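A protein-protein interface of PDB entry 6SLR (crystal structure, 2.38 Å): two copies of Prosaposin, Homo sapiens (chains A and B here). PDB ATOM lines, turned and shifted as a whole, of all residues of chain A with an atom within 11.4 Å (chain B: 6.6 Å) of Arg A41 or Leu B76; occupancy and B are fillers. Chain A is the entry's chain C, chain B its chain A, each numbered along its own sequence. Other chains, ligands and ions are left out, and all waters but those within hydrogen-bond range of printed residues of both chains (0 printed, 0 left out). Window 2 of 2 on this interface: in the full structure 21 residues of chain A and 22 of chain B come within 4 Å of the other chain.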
ATOM      1  N   ALA A  30     -21.964 -15.002  35.552  1.00  0.00           N
ATOM      2  CA  ALA A  30     -23.347 -14.512  35.748  1.00  0.00           C
ATOM      3  C   ALA A  30     -23.540 -13.200  34.975  1.00  0.00           C
ATOM      4  O   ALA A  30     -24.535 -13.088  34.215  1.00  0.00           O
ATOM      5  CB  ALA A  30     -23.631 -14.341  37.217  1.00  0.00           C
ATOM      6  N   LEU A  31     -22.611 -12.253  35.130  1.00  0.00           N
ATOM      7  CA  LEU A  31     -22.713 -10.928  34.475  1.00  0.00           C
ATOM      8  C   LEU A  31     -22.773 -11.130  32.963  1.00  0.00           C
ATOM      9  O   LEU A  31     -23.691 -10.567  32.327  1.00  0.00           O
ATOM     10  CB  LEU A  31     -21.518 -10.058  34.868  1.00  0.00           C
ATOM     11  CG  LEU A  31     -21.546  -8.628  34.334  1.00  0.00           C
ATOM     12  CD1 LEU A  31     -22.765  -7.860  34.852  1.00  0.00           C
ATOM     13  CD2 LEU A  31     -20.258  -7.909  34.705  1.00  0.00           C
ATOM     14  N   VAL A  32     -21.849 -11.921  32.415  1.00  0.00           N
ATOM     15  CA  VAL A  32     -21.710 -12.102  30.943  1.00  0.00           C
ATOM     16  C   VAL A  32     -23.005 -12.722  30.413  1.00  0.00           C
ATOM     17  O   VAL A  32     -23.469 -12.266  29.368  1.00  0.00           O
ATOM     18  CB  VAL A  32     -20.455 -12.922  30.561  1.00  0.00           C
ATOM     19  CG1 VAL A  32     -19.168 -12.281  31.075  1.00  0.00           C
ATOM     20  CG2 VAL A  32     -20.534 -14.374  31.000  1.00  0.00           C
ATOM     21  N   GLU A  33     -23.586 -13.694  31.118  1.00  0.00           N
ATOM     22  CA  GLU A  33     -24.816 -14.390  30.657  1.00  0.00           C
ATOM     23  C   GLU A  33     -25.985 -13.400  30.717  1.00  0.00           C
ATOM     24  O   GLU A  33     -26.775 -13.350  29.747  1.00  0.00           O
ATOM     25  CB  GLU A  33     -25.056 -15.686  31.440  1.00  0.00           C
ATOM     26  CG  GLU A  33     -25.486 -15.516  32.887  1.00  0.00           C
ATOM     27  CD  GLU A  33     -26.930 -15.074  33.099  1.00  0.00           C
ATOM     28  OE1 GLU A  33     -27.779 -15.387  32.234  1.00  0.00           O
ATOM     29  OE2 GLU A  33     -27.210 -14.414  34.129  1.00  0.00           O
ATOM     30  N   HIS A  34     -26.071 -12.613  31.789  1.00  0.00           N
ATOM     31  CA  HIS A  34     -27.133 -11.592  31.952  1.00  0.00           C
ATOM     32  C   HIS A  34     -27.102 -10.634  30.759  1.00  0.00           C
ATOM     33  O   HIS A  34     -28.166 -10.388  30.149  1.00  0.00           O
ATOM     34  CB  HIS A  34     -26.980 -10.822  33.260  1.00  0.00           C
ATOM     35  CG  HIS A  34     -28.018  -9.761  33.370  1.00  0.00           C
ATOM     36  ND1 HIS A  34     -29.338 -10.050  33.664  1.00  0.00           N
ATOM     37  CD2 HIS A  34     -27.960  -8.433  33.155  1.00  0.00           C
ATOM     38  CE1 HIS A  34     -30.037  -8.938  33.659  1.00  0.00           C
ATOM     39  NE2 HIS A  34     -29.215  -7.934  33.352  1.00  0.00           N
ATOM     40  N   VAL A  35     -25.919 -10.118  30.437  1.00  0.00           N
ATOM     41  CA  VAL A  35     -25.747  -9.091  29.372  1.00  0.00           C
ATOM     42  C   VAL A  35     -26.154  -9.707  28.028  1.00  0.00           C
ATOM     43  O   VAL A  35     -26.799  -9.005  27.235  1.00  0.00           O
ATOM     44  CB  VAL A  35     -24.311  -8.532  29.370  1.00  0.00           C
ATOM     45  CG1 VAL A  35     -23.984  -7.761  28.095  1.00  0.00           C
ATOM     46  CG2 VAL A  35     -24.051  -7.679  30.609  1.00  0.00           C
ATOM     47  N   LYS A  36     -25.821 -10.976  27.786  1.00  0.00           N
ATOM     48  CA  LYS A  36     -26.224 -11.706  26.555  1.00  0.00           C
ATOM     49  C   LYS A  36     -27.755 -11.728  26.447  1.00  0.00           C
ATOM     50  O   LYS A  36     -28.272 -11.509  25.344  1.00  0.00           O
ATOM     51  CB  LYS A  36     -25.668 -13.133  26.551  1.00  0.00           C
ATOM     52  CG  LYS A  36     -24.186 -13.251  26.249  1.00  0.00           C
ATOM     53  CD  LYS A  36     -23.696 -14.682  26.232  1.00  0.00           C
ATOM     54  CE  LYS A  36     -22.204 -14.772  26.008  1.00  0.00           C
ATOM     55  NZ  LYS A  36     -21.771 -16.169  25.776  1.00  0.00           N
ATOM     56  N   GLU A  37     -28.460 -11.971  27.551  1.00  0.00           N
ATOM     57  CA  GLU A  37     -29.948 -12.031  27.570  1.00  0.00           C
ATOM     58  C   GLU A  37     -30.523 -10.657  27.195  1.00  0.00           C
ATOM     59  O   GLU A  37     -31.515 -10.605  26.460  1.00  0.00           O
ATOM     60  CB  GLU A  37     -30.443 -12.536  28.927  1.00  0.00           C
ATOM     61  CG  GLU A  37     -30.055 -13.990  29.179  1.00  0.00           C
ATOM     62  CD  GLU A  37     -30.918 -14.767  30.157  1.00  0.00           C
ATOM     63  OE1 GLU A  37     -31.531 -14.114  31.032  1.00  0.00           O
ATOM     64  OE2 GLU A  37     -30.981 -16.022  30.031  1.00  0.00           O
ATOM     65  N   GLU A  38     -29.902  -9.600  27.702  1.00  0.00           N
ATOM     66  CA  GLU A  38     -30.367  -8.218  27.448  1.00  0.00           C
ATOM     67  C   GLU A  38     -30.171  -7.880  25.975  1.00  0.00           C
ATOM     68  O   GLU A  38     -30.605  -6.818  25.553  1.00  0.00           O
ATOM     69  CB  GLU A  38     -29.631  -7.251  28.371  1.00  0.00           C
ATOM     70  CG  GLU A  38     -29.937  -7.493  29.830  1.00  0.00           C
ATOM     71  CD  GLU A  38     -31.388  -7.272  30.201  1.00  0.00           C
ATOM     72  OE1 GLU A  38     -32.149  -6.820  29.356  1.00  0.00           O
ATOM     73  OE2 GLU A  38     -31.745  -7.562  31.331  1.00  0.00           O
ATOM     74  N   CYS A  39     -29.536  -8.771  25.222  1.00  0.00           N
ATOM     75  CA  CYS A  39     -29.338  -8.531  23.770  1.00  0.00           C
ATOM     76  C   CYS A  39     -30.700  -8.493  23.053  1.00  0.00           C
ATOM     77  O   CYS A  39     -30.835  -7.723  22.092  1.00  0.00           O
ATOM     78  CB  CYS A  39     -28.350  -9.525  23.169  1.00  0.00           C
ATOM     79  SG  CYS A  39     -26.612  -9.023  23.306  1.00  0.00           S
ATOM     80  N   ASP A  40     -31.658  -9.321  23.484  1.00  0.00           N
ATOM     81  CA  ASP A  40     -33.010  -9.389  22.864  1.00  0.00           C
ATOM     82  C   ASP A  40     -33.723  -8.031  22.829  1.00  0.00           C
ATOM     83  O   ASP A  40     -34.567  -7.859  21.954  1.00  0.00           O
ATOM     84  CB  ASP A  40     -33.884 -10.454  23.522  1.00  0.00           C
ATOM     85  CG  ASP A  40     -33.105 -11.691  23.910  1.00  0.00           C
ATOM     86  OD1 ASP A  40     -31.901 -11.706  23.654  1.00  0.00           O
ATOM     87  OD2 ASP A  40     -33.683 -12.585  24.533  1.00  0.00           O
ATOM     88  N   ARG A  41     -33.419  -7.104  23.737  1.00  0.00           N
ATOM     89  CA  ARG A  41     -34.139  -5.799  23.738  1.00  0.00           C
ATOM     90  C   ARG A  41     -33.900  -5.014  22.437  1.00  0.00           C
ATOM     91  O   ARG A  41     -34.680  -4.059  22.179  1.00  0.00           O
ATOM     92  CB  ARG A  41     -33.721  -4.964  24.948  1.00  0.00           C
ATOM     93  CG  ARG A  41     -34.088  -5.609  26.274  1.00  0.00           C
ATOM     94  CD  ARG A  41     -33.877  -4.652  27.418  1.00  0.00           C
ATOM     95  NE  ARG A  41     -34.359  -5.227  28.661  1.00  0.00           N
ATOM     96  CZ  ARG A  41     -35.625  -5.251  29.058  1.00  0.00           C
ATOM     97  NH1 ARG A  41     -36.587  -4.727  28.314  1.00  0.00           N
ATOM     98  NH2 ARG A  41     -35.925  -5.816  30.210  1.00  0.00           N
ATOM     99  N   LEU A  42     -32.876  -5.383  21.652  1.00  0.00           N
ATOM    100  CA  LEU A  42     -32.554  -4.740  20.349  1.00  0.00           C
ATOM    101  C   LEU A  42     -33.444  -5.324  19.246  1.00  0.00           C
ATOM    102  O   LEU A  42     -33.550  -6.558  19.147  1.00  0.00           O
ATOM    103  CB  LEU A  42     -31.068  -4.932  20.040  1.00  0.00           C
ATOM    104  CG  LEU A  42     -30.109  -4.300  21.048  1.00  0.00           C
ATOM    105  CD1 LEU A  42     -28.664  -4.528  20.638  1.00  0.00           C
ATOM    106  CD2 LEU A  42     -30.370  -2.803  21.217  1.00  0.00           C
ATOM    107  N   GLY A  43     -34.061  -4.442  18.457  1.00  0.00           N
ATOM    108  CA  GLY A  43     -35.031  -4.794  17.399  1.00  0.00           C
ATOM    109  C   GLY A  43     -34.351  -5.161  16.090  1.00  0.00           C
ATOM    110  O   GLY A  43     -33.835  -6.292  16.021  1.00  0.00           O
ATOM    111  N   GLY A  45     -28.821  -3.319  16.775  1.00  0.00           N
ATOM    112  CA  GLY A  45     -28.995  -4.235  15.630  1.00  0.00           C
ATOM    113  C   GLY A  45     -29.814  -5.460  16.003  1.00  0.00           C
ATOM    114  O   GLY A  45     -30.835  -5.294  16.710  1.00  0.00           O
ATOM    115  N   MET A  46     -29.412  -6.636  15.503  1.00  0.00           N
ATOM    116  CA  MET A  46     -30.060  -7.931  15.824  1.00  0.00           C
ATOM    117  C   MET A  46     -29.439  -8.510  17.106  1.00  0.00           C
ATOM    118  O   MET A  46     -28.306  -8.125  17.510  1.00  0.00           O
ATOM    119  CB  MET A  46     -29.939  -8.941  14.676  1.00  0.00           C
ATOM    120  CG  MET A  46     -31.039  -9.999  14.677  1.00  0.00           C
ATOM    121  SD  MET A  46     -32.733  -9.323  14.652  1.00  0.00           S
ATOM    122  CE  MET A  46     -33.681 -10.725  15.246  1.00  0.00           C
ATOM    123  N   ALA A  47     -30.186  -9.405  17.754  1.00  0.00           N
ATOM    124  CA  ALA A  47     -29.894  -9.973  19.093  1.00  0.00           C
ATOM    125  C   ALA A  47     -28.746 -10.988  19.014  1.00  0.00           C
ATOM    126  O   ALA A  47     -27.851 -10.906  19.870  1.00  0.00           O
ATOM    127  CB  ALA A  47     -31.144 -10.605  19.650  1.00  0.00           C
ATOM    128  N   ASP A  48     -28.786 -11.930  18.061  1.00  0.00           N
ATOM    129  CA  ASP A  48     -27.753 -12.990  17.920  1.00  0.00           C
ATOM    130  C   ASP A  48     -26.425 -12.349  17.516  1.00  0.00           C
ATOM    131  O   ASP A  48     -25.387 -12.795  18.026  1.00  0.00           O
ATOM    132  CB  ASP A  48     -28.207 -14.099  16.975  1.00  0.00           C
ATOM    133  CG  ASP A  48     -28.937 -15.206  17.717  1.00  0.00           C
ATOM    134  OD1 ASP A  48     -29.442 -14.923  18.826  1.00  0.00           O
ATOM    135  OD2 ASP A  48     -28.954 -16.346  17.208  1.00  0.00           O
ATOM    136  N   ILE A  49     -26.489 -11.301  16.703  1.00  0.00           N
ATOM    137  CA  ILE A  49     -25.259 -10.546  16.344  1.00  0.00           C
ATOM    138  C   ILE A  49     -24.659 -10.083  17.672  1.00  0.00           C
ATOM    139  O   ILE A  49     -23.490 -10.381  17.951  1.00  0.00           O
ATOM    140  CB  ILE A  49     -25.636  -9.353  15.446  1.00  0.00           C
ATOM    141  CG1 ILE A  49     -25.710  -9.755  13.973  1.00  0.00           C
ATOM    142  CG2 ILE A  49     -24.697  -8.180  15.651  1.00  0.00           C
ATOM    143  CD1 ILE A  49     -26.689 -10.863  13.682  1.00  0.00           C
ATOM    144  N   CYS A  50     -25.506  -9.487  18.505  1.00  0.00           N
ATOM    145  CA  CYS A  50     -25.114  -8.919  19.813  1.00  0.00           C
ATOM    146  C   CYS A  50     -24.563 -10.039  20.696  1.00  0.00           C
ATOM    147  O   CYS A  50     -23.521  -9.835  21.298  1.00  0.00           O
ATOM    148  CB  CYS A  50     -26.368  -8.285  20.406  1.00  0.00           C
ATOM    149  SG  CYS A  50     -26.223  -7.511  22.036  1.00  0.00           S
ATOM    150  N   LYS A  51     -25.221 -11.195  20.729  1.00  0.00           N
ATOM    151  CA  LYS A  51     -24.773 -12.293  21.626  1.00  0.00           C
ATOM    152  C   LYS A  51     -23.405 -12.829  21.187  1.00  0.00           C
ATOM    153  O   LYS A  51     -22.654 -13.332  22.031  1.00  0.00           O
ATOM    154  CB  LYS A  51     -25.832 -13.397  21.673  1.00  0.00           C
ATOM    155  CG  LYS A  51     -26.939 -13.199  22.696  1.00  0.00           C
ATOM    156  CD  LYS A  51     -28.009 -14.263  22.629  1.00  0.00           C
ATOM    157  CE  LYS A  51     -28.810 -14.401  23.905  1.00  0.00           C
ATOM    158  NZ  LYS A  51     -30.236 -14.693  23.635  1.00  0.00           N
ATOM    159  N   ILE A  54     -20.505 -10.249  22.253  1.00  0.00           N
ATOM    160  CA  ILE A  54     -20.193 -10.447  23.703  1.00  0.00           C
ATOM    161  C   ILE A  54     -19.383 -11.745  23.841  1.00  0.00           C
ATOM    162  O   ILE A  54     -18.318 -11.712  24.488  1.00  0.00           O
ATOM    163  CB  ILE A  54     -21.461 -10.436  24.592  1.00  0.00           C
ATOM    164  CG1 ILE A  54     -21.935  -9.013  24.907  1.00  0.00           C
ATOM    165  CG2 ILE A  54     -21.247 -11.196  25.897  1.00  0.00           C
ATOM    166  CD1 ILE A  54     -22.700  -8.348  23.798  1.00  0.00           C
ATOM    167  N   MET B  68     -36.257   5.640  35.207  1.00  0.00           N
ATOM    168  CA  MET B  68     -36.088   4.330  35.887  1.00  0.00           C
ATOM    169  C   MET B  68     -35.505   4.570  37.281  1.00  0.00           C
ATOM    170  O   MET B  68     -34.777   5.568  37.458  1.00  0.00           O
ATOM    171  CB  MET B  68     -35.168   3.418  35.081  1.00  0.00           C
ATOM    172  CG  MET B  68     -35.783   2.911  33.781  1.00  0.00           C
ATOM    173  SD  MET B  68     -34.591   1.970  32.772  1.00  0.00           S
ATOM    174  CE  MET B  68     -34.597   0.406  33.649  1.00  0.00           C
ATOM    175  N   LYS B  71     -32.239   0.975  41.331  1.00  0.00           N
ATOM    176  CA  LYS B  71     -32.262  -0.503  41.508  1.00  0.00           C
ATOM    177  C   LYS B  71     -32.554  -1.160  40.152  1.00  0.00           C
ATOM    178  O   LYS B  71     -31.893  -2.173  39.826  1.00  0.00           O
ATOM    179  CB  LYS B  71     -33.327  -0.911  42.530  1.00  0.00           C
ATOM    180  CG  LYS B  71     -32.809  -1.668  43.742  1.00  0.00           C
ATOM    181  CD  LYS B  71     -33.898  -1.959  44.737  1.00  0.00           C
ATOM    182  CE  LYS B  71     -33.374  -2.664  45.967  1.00  0.00           C
ATOM    183  NZ  LYS B  71     -34.467  -2.947  46.930  1.00  0.00           N
ATOM    184  N   GLU B  72     -33.525  -0.600  39.418  1.00  0.00           N
ATOM    185  CA  GLU B  72     -33.994  -1.111  38.100  1.00  0.00           C
ATOM    186  C   GLU B  72     -32.838  -1.038  37.099  1.00  0.00           C
ATOM    187  O   GLU B  72     -32.653  -1.999  36.347  1.00  0.00           O
ATOM    188  CB  GLU B  72     -35.179  -0.299  37.560  1.00  0.00           C
ATOM    189  CG  GLU B  72     -36.481  -0.501  38.309  1.00  0.00           C
ATOM    190  CD  GLU B  72     -37.629   0.407  37.876  1.00  0.00           C
ATOM    191  OE1 GLU B  72     -37.381   1.516  37.358  1.00  0.00           O
ATOM    192  OE2 GLU B  72     -38.788   0.010  38.066  1.00  0.00           O
ATOM    193  N   ILE B  73     -32.114   0.078  37.085  1.00  0.00           N
ATOM    194  CA  ILE B  73     -30.974   0.310  36.153  1.00  0.00           C
ATOM    195  C   ILE B  73     -29.869  -0.704  36.480  1.00  0.00           C
ATOM    196  O   ILE B  73     -29.360  -1.361  35.550  1.00  0.00           O
ATOM    197  CB  ILE B  73     -30.498   1.771  36.246  1.00  0.00           C
ATOM    198  CG1 ILE B  73     -31.570   2.734  35.731  1.00  0.00           C
ATOM    199  CG2 ILE B  73     -29.175   1.963  35.518  1.00  0.00           C
ATOM    200  CD1 ILE B  73     -31.409   4.165  36.216  1.00  0.00           C
ATOM    201  N   CYS B  74     -29.551  -0.863  37.759  1.00  0.00           N
ATOM    202  CA  CYS B  74     -28.467  -1.757  38.246  1.00  0.00           C
ATOM    203  C   CYS B  74     -28.810  -3.222  37.955  1.00  0.00           C
ATOM    204  O   CYS B  74     -27.917  -3.955  37.458  1.00  0.00           O
ATOM    205  CB  CYS B  74     -28.196  -1.498  39.718  1.00  0.00           C
ATOM    206  SG  CYS B  74     -27.435   0.129  39.944  1.00  0.00           S
ATOM    207  N   ALA B  75     -30.064  -3.611  38.183  1.00  0.00           N
ATOM    208  CA  ALA B  75     -30.583  -4.941  37.780  1.00  0.00           C
ATOM    209  C   ALA B  75     -30.469  -5.108  36.255  1.00  0.00           C
ATOM    210  O   ALA B  75     -30.016  -6.172  35.797  1.00  0.00           O
ATOM    211  CB  ALA B  75     -32.003  -5.124  38.251  1.00  0.00           C
ATOM    212  N   LEU B  76     -30.855  -4.086  35.492  1.00  0.00           N
ATOM    213  CA  LEU B  76     -30.814  -4.121  34.010  1.00  0.00           C
ATOM    214  C   LEU B  76     -29.386  -4.422  33.545  1.00  0.00           C
ATOM    215  O   LEU B  76     -29.226  -5.269  32.670  1.00  0.00           O
ATOM    216  CB  LEU B  76     -31.296  -2.782  33.447  1.00  0.00           C
ATOM    217  CG  LEU B  76     -31.243  -2.670  31.929  1.00  0.00           C
ATOM    218  CD1 LEU B  76     -32.077  -3.778  31.295  1.00  0.00           C
ATOM    219  CD2 LEU B  76     -31.715  -1.293  31.479  1.00  0.00           C
ATOM    220  N   VAL B  77     -28.385  -3.760  34.116  1.00  0.00           N
ATOM    221  CA  VAL B  77     -26.963  -3.942  33.705  1.00  0.00           C
ATOM    222  C   VAL B  77     -26.410  -5.248  34.285  1.00  0.00           C
ATOM    223  O   VAL B  77     -25.430  -5.756  33.719  1.00  0.00           O
ATOM    224  CB  VAL B  77     -26.115  -2.724  34.104  1.00  0.00           C
ATOM    225  CG1 VAL B  77     -24.638  -2.945  33.832  1.00  0.00           C
ATOM    226  CG2 VAL B  77     -26.606  -1.477  33.385  1.00  0.00           C
ATOM    227  N   GLY B  78     -27.007  -5.777  35.358  1.00  0.00           N
ATOM    228  CA  GLY B  78     -26.645  -7.090  35.931  1.00  0.00           C
ATOM    229  C   GLY B  78     -25.788  -6.994  37.184  1.00  0.00           C
ATOM    230  O   GLY B  78     -25.352  -8.048  37.647  1.00  0.00           O
ATOM    231  N   PHE B  79     -25.590  -5.798  37.747  1.00  0.00           N
ATOM    232  CA  PHE B  79     -24.839  -5.582  39.012  1.00  0.00           C
ATOM    233  C   PHE B  79     -25.723  -5.820  40.248  1.00  0.00           C
ATOM    234  O   PHE B  79     -25.154  -5.868  41.362  1.00  0.00           O
ATOM    235  CB  PHE B  79     -24.234  -4.176  39.052  1.00  0.00           C
ATOM    236  CG  PHE B  79     -23.172  -3.914  38.015  1.00  0.00           C
ATOM    237  CD1 PHE B  79     -22.270  -4.904  37.642  1.00  0.00           C
ATOM    238  CD2 PHE B  79     -23.048  -2.660  37.441  1.00  0.00           C
ATOM    239  CE1 PHE B  79     -21.287  -4.645  36.703  1.00  0.00           C
ATOM    240  CE2 PHE B  79     -22.073  -2.406  36.489  1.00  0.00           C
ATOM    241  CZ  PHE B  79     -21.191  -3.400  36.126  1.00  0.00           C
ATOM    242  N   CYS B  80     -27.048  -5.929  40.081  1.00  0.00           N
ATOM    243  CA  CYS B  80     -28.015  -6.257  41.167  1.00  0.00           C
ATOM    244  C   CYS B  80     -28.866  -7.463  40.751  1.00  0.00           C
ATOM    245  O   CYS B  80     -29.197  -7.559  39.559  1.00  0.00           O
ATOM    246  CB  CYS B  80     -28.920  -5.072  41.498  1.00  0.00           C
ATOM    247  SG  CYS B  80     -28.096  -3.725  42.398  1.00  0.00           S
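A ring nitrogen (NE2) of His A34 is in hydrogen-bond range of the backbone carbonyl oxygen (O) of Leu B76.
O of Ala B75 lies within hydrogen-bond range of NE2 of His A34, 3.1 Å away.
N of Phe B79 sits at hydrogen-bond distance from O of Cys B74.
The side-chain carboxylate of Glu A38 is in salt-bridge range of the guanidinium group of Arg A41 (2.8 Å).
The side-chain sulfur (SG) of Cys A39 is disulfide-bonded to the side-chain sulfur (SG) of Cys A50, 2.0 Å away.
NE2 of His A34 lies close to OE2 of Glu A38, 3.3 Å away.
Leu A31 touches Val B77 (CD1 to O, 3.6 Å).
O of Gly B78 touches CD1 of Leu A31 (3.8 Å).
CE1 of Phe B79 touches CD2 of Leu A31, at 3.96 Å.
CD2 of His A34 touches C of Val B77, 3.7 Å away.
His A34 touches Gly B78.
Val A35 touches Val B77.
CD1 of Leu B76 touches OE1 of Glu A38 (3.6 Å).
Leu B76 touches Arg A41.
Of the printed residues of chain B, Arg A41 touches Leu B76.
Leu B76 touches just these residues of chain A: His A34 (2.8 Å), Glu A38 (3.6 Å) and Arg A41 (3.8 Å).
No residue of chain A comes within 4 Å of Cys B74.
Val B77 touches just these residues of chain A: Leu A31 (3.6 Å), His A34 (3.7 Å) and Val A35 (3.9 Å).
Gly B78 touches two residues of chain A.
Printed residues of chain A within 4 Å of Phe B79: Leu A31 (3.96 Å).
Of the printed residues of chain B, Glu A38 touches Leu B76.
Printed residues of chain B within 4 Å of Leu A31: Val B77 (3.6 Å), Gly B78 (3.8 Å) and Phe B79 (3.96 Å).
Cys A39 touches none of the printed residues of chain B.
Glu A33 touches none of the printed residues of chain B.
The nearest printed residue of chain B that does not touch Arg A41 is Met B68 (7.2 Å).
The nearest residue of chain A that does not touch Leu B76 is Val A35 (6.1 Å).
Printed residues of chain A that touch a printed residue of chain B: Leu A31, His A34, Val A35, Glu A38 and Arg A41.
Hydrophobic or aromatic side chains of chain A within 4 Å of the printed part of chain B: Leu A31, His A34 and Val A35.
Along chain A the printed residues that touch a printed residue of chain B span positions 31 to 41.
Of the 11 printed residues of chain B, 5 touch a printed residue of chain A.
Hydrophobic or aromatic side chains of chain B within 4 Å of the printed part of chain A: Leu B76 and Phe B79.
Among the printed residues, no Asp or Glu carboxylate lies within 4 Å of a Lys or Arg side-chain nitrogen of the other chain.
No position is printed for both chains.
Of the 10 pairs that touch across the chains among the printed residues, none has its exchanged pair printed and touching as well.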
